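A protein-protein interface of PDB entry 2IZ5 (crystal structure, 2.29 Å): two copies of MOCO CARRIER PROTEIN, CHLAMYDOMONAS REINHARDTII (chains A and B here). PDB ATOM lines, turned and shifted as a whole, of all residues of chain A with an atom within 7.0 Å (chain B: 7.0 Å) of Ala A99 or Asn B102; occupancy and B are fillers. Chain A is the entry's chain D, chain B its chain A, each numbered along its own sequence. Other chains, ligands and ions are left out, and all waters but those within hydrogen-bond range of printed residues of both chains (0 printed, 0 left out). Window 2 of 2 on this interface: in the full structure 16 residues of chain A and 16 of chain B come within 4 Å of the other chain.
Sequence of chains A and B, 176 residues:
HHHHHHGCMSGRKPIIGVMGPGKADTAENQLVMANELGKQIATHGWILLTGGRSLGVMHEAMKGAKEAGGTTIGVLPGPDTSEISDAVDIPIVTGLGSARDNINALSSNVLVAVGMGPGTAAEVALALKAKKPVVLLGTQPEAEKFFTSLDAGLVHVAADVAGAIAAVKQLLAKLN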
ATOM      1  N   PRO A  77       1.007 -11.170 -13.812  1.00  0.00           N
ATOM      2  CA  PRO A  77       1.671 -12.087 -12.856  1.00  0.00           C
ATOM      3  C   PRO A  77       0.929 -12.243 -11.533  1.00  0.00           C
ATOM      4  O   PRO A  77       0.713 -13.351 -11.094  1.00  0.00           O
ATOM      5  CB  PRO A  77       3.014 -11.400 -12.610  1.00  0.00           C
ATOM      6  CG  PRO A  77       3.267 -10.651 -13.846  1.00  0.00           C
ATOM      7  CD  PRO A  77       1.937 -10.097 -14.236  1.00  0.00           C
ATOM      8  N   THR A  94      -1.698 -15.032 -14.625  1.00  0.00           N
ATOM      9  CA  THR A  94      -0.975 -16.202 -15.191  1.00  0.00           C
ATOM     10  C   THR A  94      -0.087 -16.909 -14.150  1.00  0.00           C
ATOM     11  O   THR A  94       0.208 -18.116 -14.245  1.00  0.00           O
ATOM     12  CB  THR A  94      -0.093 -15.807 -16.453  1.00  0.00           C
ATOM     13  OG1 THR A  94       1.037 -15.023 -16.046  1.00  0.00           O
ATOM     14  CG2 THR A  94      -0.901 -15.051 -17.492  1.00  0.00           C
ATOM     15  N   GLY A  95       0.359 -16.129 -13.172  1.00  0.00           N
ATOM     16  CA  GLY A  95       1.325 -16.609 -12.199  1.00  0.00           C
ATOM     17  C   GLY A  95       2.745 -16.635 -12.751  1.00  0.00           C
ATOM     18  O   GLY A  95       3.696 -16.744 -11.975  1.00  0.00           O
ATOM     19  N   LEU A  96       2.917 -16.489 -14.071  1.00  0.00           N
ATOM     20  CA  LEU A  96       4.177 -16.891 -14.729  1.00  0.00           C
ATOM     21  C   LEU A  96       5.375 -15.988 -14.422  1.00  0.00           C
ATOM     22  O   LEU A  96       6.375 -16.076 -15.129  1.00  0.00           O
ATOM     23  CB  LEU A  96       4.013 -16.977 -16.263  1.00  0.00           C
ATOM     24  CG  LEU A  96       3.029 -17.986 -16.848  1.00  0.00           C
ATOM     25  CD1 LEU A  96       3.058 -17.994 -18.354  1.00  0.00           C
ATOM     26  CD2 LEU A  96       3.323 -19.348 -16.333  1.00  0.00           C
ATOM     27  N   GLY A  97       5.282 -15.135 -13.398  1.00  0.00           N
ATOM     28  CA  GLY A  97       6.364 -14.210 -13.055  1.00  0.00           C
ATOM     29  C   GLY A  97       7.014 -13.549 -14.266  1.00  0.00           C
ATOM     30  O   GLY A  97       6.328 -12.890 -15.067  1.00  0.00           O
ATOM     31  N   SER A  98       8.331 -13.765 -14.406  1.00  0.00           N
ATOM     32  CA  SER A  98       9.140 -13.210 -15.511  1.00  0.00           C
ATOM     33  C   SER A  98       9.035 -13.954 -16.870  1.00  0.00           C
ATOM     34  O   SER A  98       9.621 -13.503 -17.865  1.00  0.00           O
ATOM     35  CB  SER A  98      10.626 -13.096 -15.083  1.00  0.00           C
ATOM     36  OG  SER A  98      10.921 -13.883 -13.928  1.00  0.00           O
ATOM     37  N   ALA A  99       8.303 -15.062 -16.892  1.00  0.00           N
ATOM     38  CA  ALA A  99       8.170 -15.869 -18.099  1.00  0.00           C
ATOM     39  C   ALA A  99       6.961 -15.435 -18.921  1.00  0.00           C
ATOM     40  O   ALA A  99       6.308 -14.440 -18.606  1.00  0.00           O
ATOM     41  CB  ALA A  99       8.070 -17.344 -17.743  1.00  0.00           C
ATOM     42  N   ARG A 100       6.669 -16.189 -19.977  1.00  0.00           N
ATOM     43  CA  ARG A 100       5.993 -15.640 -21.147  1.00  0.00           C
ATOM     44  C   ARG A 100       4.478 -15.699 -20.987  1.00  0.00           C
ATOM     45  O   ARG A 100       3.855 -16.724 -21.263  1.00  0.00           O
ATOM     46  CB  ARG A 100       6.419 -16.388 -22.411  1.00  0.00           C
ATOM     47  CG  ARG A 100       6.940 -15.488 -23.519  1.00  0.00           C
ATOM     48  CD  ARG A 100       8.176 -14.690 -23.140  1.00  0.00           C
ATOM     49  NE  ARG A 100       8.106 -13.312 -23.619  1.00  0.00           N
ATOM     50  CZ  ARG A 100       7.959 -12.255 -22.831  1.00  0.00           C
ATOM     51  NH1 ARG A 100       7.867 -12.413 -21.517  1.00  0.00           N
ATOM     52  NH2 ARG A 100       7.904 -11.038 -23.353  1.00  0.00           N
ATOM     53  N   ASP A 101       3.891 -14.593 -20.540  1.00  0.00           N
ATOM     54  CA  ASP A 101       2.620 -14.128 -21.081  1.00  0.00           C
ATOM     55  C   ASP A 101       2.802 -13.502 -22.458  1.00  0.00           C
ATOM     56  O   ASP A 101       2.460 -12.340 -22.674  1.00  0.00           O
ATOM     57  CB  ASP A 101       1.968 -13.123 -20.128  1.00  0.00           C
ATOM     58  CG  ASP A 101       2.208 -13.461 -18.670  1.00  0.00           C
ATOM     59  OD1 ASP A 101       2.620 -14.605 -18.384  1.00  0.00           O
ATOM     60  OD2 ASP A 101       2.014 -12.648 -17.742  1.00  0.00           O
ATOM     61  N   ASN A 102       3.342 -14.281 -23.390  1.00  0.00           N
ATOM     62  CA  ASN A 102       2.919 -14.216 -24.784  1.00  0.00           C
ATOM     63  C   ASN A 102       1.449 -14.580 -24.956  1.00  0.00           C
ATOM     64  O   ASN A 102       1.056 -15.150 -25.974  1.00  0.00           O
ATOM     65  CB  ASN A 102       3.791 -15.126 -25.651  1.00  0.00           C
ATOM     66  CG  ASN A 102       3.273 -16.549 -25.707  1.00  0.00           C
ATOM     67  OD1 ASN A 102       3.027 -17.091 -26.785  1.00  0.00           O
ATOM     68  ND2 ASN A 102       3.104 -17.164 -24.543  1.00  0.00           N
ATOM     69  N   VAL B  75      16.723 -28.276 -24.467  1.00  0.00           N
ATOM     70  CA  VAL B  75      15.420 -27.842 -23.968  1.00  0.00           C
ATOM     71  C   VAL B  75      14.377 -28.069 -25.085  1.00  0.00           C
ATOM     72  O   VAL B  75      14.638 -27.724 -26.234  1.00  0.00           O
ATOM     73  CB  VAL B  75      15.474 -26.363 -23.481  1.00  0.00           C
ATOM     74  CG1 VAL B  75      14.166 -25.955 -22.810  1.00  0.00           C
ATOM     75  CG2 VAL B  75      16.634 -26.172 -22.515  1.00  0.00           C
ATOM     76  N   LEU B  96       5.922 -26.333 -22.992  1.00  0.00           N
ATOM     77  CA  LEU B  96       5.475 -24.970 -23.212  1.00  0.00           C
ATOM     78  C   LEU B  96       5.654 -24.719 -24.707  1.00  0.00           C
ATOM     79  O   LEU B  96       6.638 -24.074 -25.118  1.00  0.00           O
ATOM     80  CB  LEU B  96       6.353 -24.002 -22.398  1.00  0.00           C
ATOM     81  CG  LEU B  96       6.444 -24.200 -20.886  1.00  0.00           C
ATOM     82  CD1 LEU B  96       7.754 -23.624 -20.336  1.00  0.00           C
ATOM     83  CD2 LEU B  96       5.217 -23.586 -20.216  1.00  0.00           C
ATOM     84  N   ALA B  99       4.786 -20.810 -26.752  1.00  0.00           N
ATOM     85  CA  ALA B  99       5.175 -20.462 -25.378  1.00  0.00           C
ATOM     86  C   ALA B  99       6.630 -19.999 -25.296  1.00  0.00           C
ATOM     87  O   ALA B  99       7.178 -19.575 -26.298  1.00  0.00           O
ATOM     88  CB  ALA B  99       4.962 -21.632 -24.472  1.00  0.00           C
ATOM     89  N   ARG B 100       7.250 -20.055 -24.115  1.00  0.00           N
ATOM     90  CA  ARG B 100       8.651 -19.652 -24.012  1.00  0.00           C
ATOM     91  C   ARG B 100       9.507 -20.340 -22.923  1.00  0.00           C
ATOM     92  O   ARG B 100       9.468 -19.999 -21.735  1.00  0.00           O
ATOM     93  CB  ARG B 100       8.756 -18.142 -23.855  1.00  0.00           C
ATOM     94  CG  ARG B 100      10.027 -17.567 -24.448  1.00  0.00           C
ATOM     95  CD  ARG B 100       9.761 -16.936 -25.788  1.00  0.00           C
ATOM     96  NE  ARG B 100      10.906 -16.997 -26.707  1.00  0.00           N
ATOM     97  CZ  ARG B 100      11.088 -17.928 -27.650  1.00  0.00           C
ATOM     98  NH1 ARG B 100      10.215 -18.937 -27.809  1.00  0.00           N
ATOM     99  NH2 ARG B 100      12.155 -17.853 -28.443  1.00  0.00           N
ATOM    100  N   ASP B 101      10.306 -21.307 -23.365  1.00  0.00           N
ATOM    101  CA  ASP B 101      11.542 -21.630 -22.681  1.00  0.00           C
ATOM    102  C   ASP B 101      12.227 -20.215 -22.593  1.00  0.00           C
ATOM    103  O   ASP B 101      12.581 -19.603 -23.610  1.00  0.00           O
ATOM    104  CB  ASP B 101      12.280 -22.738 -23.472  1.00  0.00           C
ATOM    105  CG  ASP B 101      11.262 -23.796 -24.114  1.00  0.00           C
ATOM    106  OD1 ASP B 101      10.166 -23.979 -23.533  1.00  0.00           O
ATOM    107  OD2 ASP B 101      11.517 -24.416 -25.198  1.00  0.00           O
ATOM    108  N   ASN B 102      12.183 -19.653 -21.371  1.00  0.00           N
ATOM    109  CA  ASN B 102      12.980 -18.507 -20.879  1.00  0.00           C
ATOM    110  C   ASN B 102      14.212 -19.073 -20.111  1.00  0.00           C
ATOM    111  O   ASN B 102      14.801 -18.430 -19.233  1.00  0.00           O
ATOM    112  CB  ASN B 102      12.157 -17.708 -19.847  1.00  0.00           C
ATOM    113  CG  ASN B 102      10.989 -16.899 -20.456  1.00  0.00           C
ATOM    114  OD1 ASN B 102      10.327 -17.318 -21.412  1.00  0.00           O
ATOM    115  ND2 ASN B 102      10.725 -15.736 -19.865  1.00  0.00           N
ATOM    116  N   ILE B 103      14.549 -20.314 -20.432  1.00  0.00           N
ATOM    117  CA  ILE B 103      15.382 -21.189 -19.603  1.00  0.00           C
ATOM    118  C   ILE B 103      16.843 -20.938 -19.930  1.00  0.00           C
ATOM    119  O   ILE B 103      17.691 -20.759 -19.058  1.00  0.00           O
ATOM    120  CB  ILE B 103      14.945 -22.697 -19.841  1.00  0.00           C
ATOM    121  CG1 ILE B 103      13.630 -22.971 -19.065  1.00  0.00           C
ATOM    122  CG2 ILE B 103      16.047 -23.680 -19.459  1.00  0.00           C
ATOM    123  CD1 ILE B 103      12.928 -24.288 -19.389  1.00  0.00           C
ATOM    124  N   ASN B 104      17.094 -20.862 -21.217  1.00  0.00           N
ATOM    125  CA  ASN B 104      18.397 -20.505 -21.759  1.00  0.00           C
ATOM    126  C   ASN B 104      18.834 -19.198 -21.129  1.00  0.00           C
ATOM    127  O   ASN B 104      19.869 -19.142 -20.461  1.00  0.00           O
ATOM    128  CB  ASN B 104      18.335 -20.434 -23.291  1.00  0.00           C
ATOM    129  CG  ASN B 104      19.727 -20.667 -23.985  1.00  0.00           C
ATOM    130  OD1 ASN B 104      20.748 -20.236 -23.472  1.00  0.00           O
ATOM    131  ND2 ASN B 104      19.728 -21.324 -25.186  1.00  0.00           N
ATOM    132  N   ALA B 105      18.015 -18.168 -21.311  1.00  0.00           N
ATOM    133  CA  ALA B 105      18.350 -16.828 -20.878  1.00  0.00           C
ATOM    134  C   ALA B 105      18.712 -16.854 -19.424  1.00  0.00           C
ATOM    135  O   ALA B 105      19.788 -16.374 -19.056  1.00  0.00           O
ATOM    136  CB  ALA B 105      17.153 -15.880 -21.109  1.00  0.00           C
ATOM    137  N   LEU B 106      17.826 -17.444 -18.596  1.00  0.00           N
ATOM    138  CA  LEU B 106      18.007 -17.423 -17.122  1.00  0.00           C
ATOM    139  C   LEU B 106      18.985 -18.451 -16.532  1.00  0.00           C
ATOM    140  O   LEU B 106      19.594 -18.181 -15.493  1.00  0.00           O
ATOM    141  CB  LEU B 106      16.658 -17.508 -16.432  1.00  0.00           C
ATOM    142  CG  LEU B 106      15.516 -16.591 -16.940  1.00  0.00           C
ATOM    143  CD1 LEU B 106      14.267 -16.678 -16.036  1.00  0.00           C
ATOM    144  CD2 LEU B 106      15.957 -15.160 -17.092  1.00  0.00           C
ATOM    145  N   SER B 107      19.180 -19.601 -17.186  1.00  0.00           N
ATOM    146  CA  SER B 107      20.111 -20.649 -16.655  1.00  0.00           C
ATOM    147  C   SER B 107      21.612 -20.515 -17.073  1.00  0.00           C
ATOM    148  O   SER B 107      22.530 -20.981 -16.372  1.00  0.00           O
ATOM    149  CB  SER B 107      19.605 -22.033 -17.044  1.00  0.00           C
ATOM    150  OG  SER B 107      18.201 -22.126 -16.867  1.00  0.00           O
ATOM    151  N   GLU B 123      14.636 -14.434 -27.595  1.00  0.00           N
ATOM    152  CA  GLU B 123      15.557 -15.037 -26.611  1.00  0.00           C
ATOM    153  C   GLU B 123      16.637 -14.020 -26.195  1.00  0.00           C
ATOM    154  O   GLU B 123      16.899 -13.826 -25.010  1.00  0.00           O
ATOM    155  CB  GLU B 123      16.227 -16.304 -27.182  1.00  0.00           C
ATOM    156  CG  GLU B 123      15.499 -17.684 -27.077  1.00  0.00           C
ATOM    157  CD  GLU B 123      16.299 -18.801 -27.861  1.00  0.00           C
ATOM    158  OE1 GLU B 123      17.025 -18.452 -28.806  1.00  0.00           O
ATOM    159  OE2 GLU B 123      16.247 -20.012 -27.561  1.00  0.00           O
ATOM    160  N   LEU B 126      15.081 -11.224 -24.195  1.00  0.00           N
ATOM    161  CA  LEU B 126      14.798 -11.753 -22.857  1.00  0.00           C
ATOM    162  C   LEU B 126      16.053 -11.916 -21.993  1.00  0.00           C
ATOM    163  O   LEU B 126      16.022 -11.662 -20.798  1.00  0.00           O
ATOM    164  CB  LEU B 126      14.014 -13.086 -22.935  1.00  0.00           C
ATOM    165  CG  LEU B 126      12.546 -12.963 -23.312  1.00  0.00           C
ATOM    166  CD1 LEU B 126      11.951 -14.323 -23.693  1.00  0.00           C
ATOM    167  CD2 LEU B 126      11.758 -12.318 -22.192  1.00  0.00           C
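Of the 13 printed residues of chain B, 4 touch a printed residue of chain A. Printed residues of chain B that touch a printed residue of chain A: Ala B99, Arg B100, Asn B102 and Leu B126. Of the 10 printed residues of chain A, 4 touch a printed residue of chain B. Among the printed residues, 6 pairs touch across the chains.
O of Arg B100 lies close to OD1 of Asn B102 (2.8 Å). The backbone carbonyl oxygen (O) of Arg A100 lies within hydrogen-bond range of the side-chain amide nitrogen (ND2) of Asn A102, at 3.4 Å.
Ala A99 touches just one residue of chain B: Asn B102 (3.1 Å). Asn B102 touches just these residues of chain A: Ser A98 (3.2 Å), Ala A99 (3.1 Å) and Arg A100 (3.8 Å). Of the printed residues of chain A, Leu B126 touches Arg A100. Of the printed residues of chain B, Asn A102 touches Ala B99. Of the printed residues of chain B, Arg A100 touches Arg B100, Asn B102 and Leu B126. Gly A95 touches none of the printed residues of chain B. Ile B103 touches none of the printed residues of chain A. The nearest printed residue of chain B that does not touch Arg A100 is Ala B99 (4.6 Å).
The side-chain amide nitrogen (ND2) of Asn B102 is in hydrogen-bond range of the backbone carbonyl oxygen (O) of Ser A98, at 3.2 Å.
Ala A99 touches Asn B102, and with the chains exchanged Asn A102 touches Ala B99. Arg B100 touches its own counterpart, Arg A100. Arg A100 touches Asn B102, but with the chains exchanged Asn A102 does not touch Arg B100 (5.1 Å). Positions printed for both chains: 96, 99, 100, 101 and 102.
Asn B102 touches Ala A99. Arg B100 touches Arg A100. Asn B102 touches Arg A100 (OD1 to CD, 3.8 Å). Arg A100 touches Leu B126. Asn A102 touches Ala B99.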
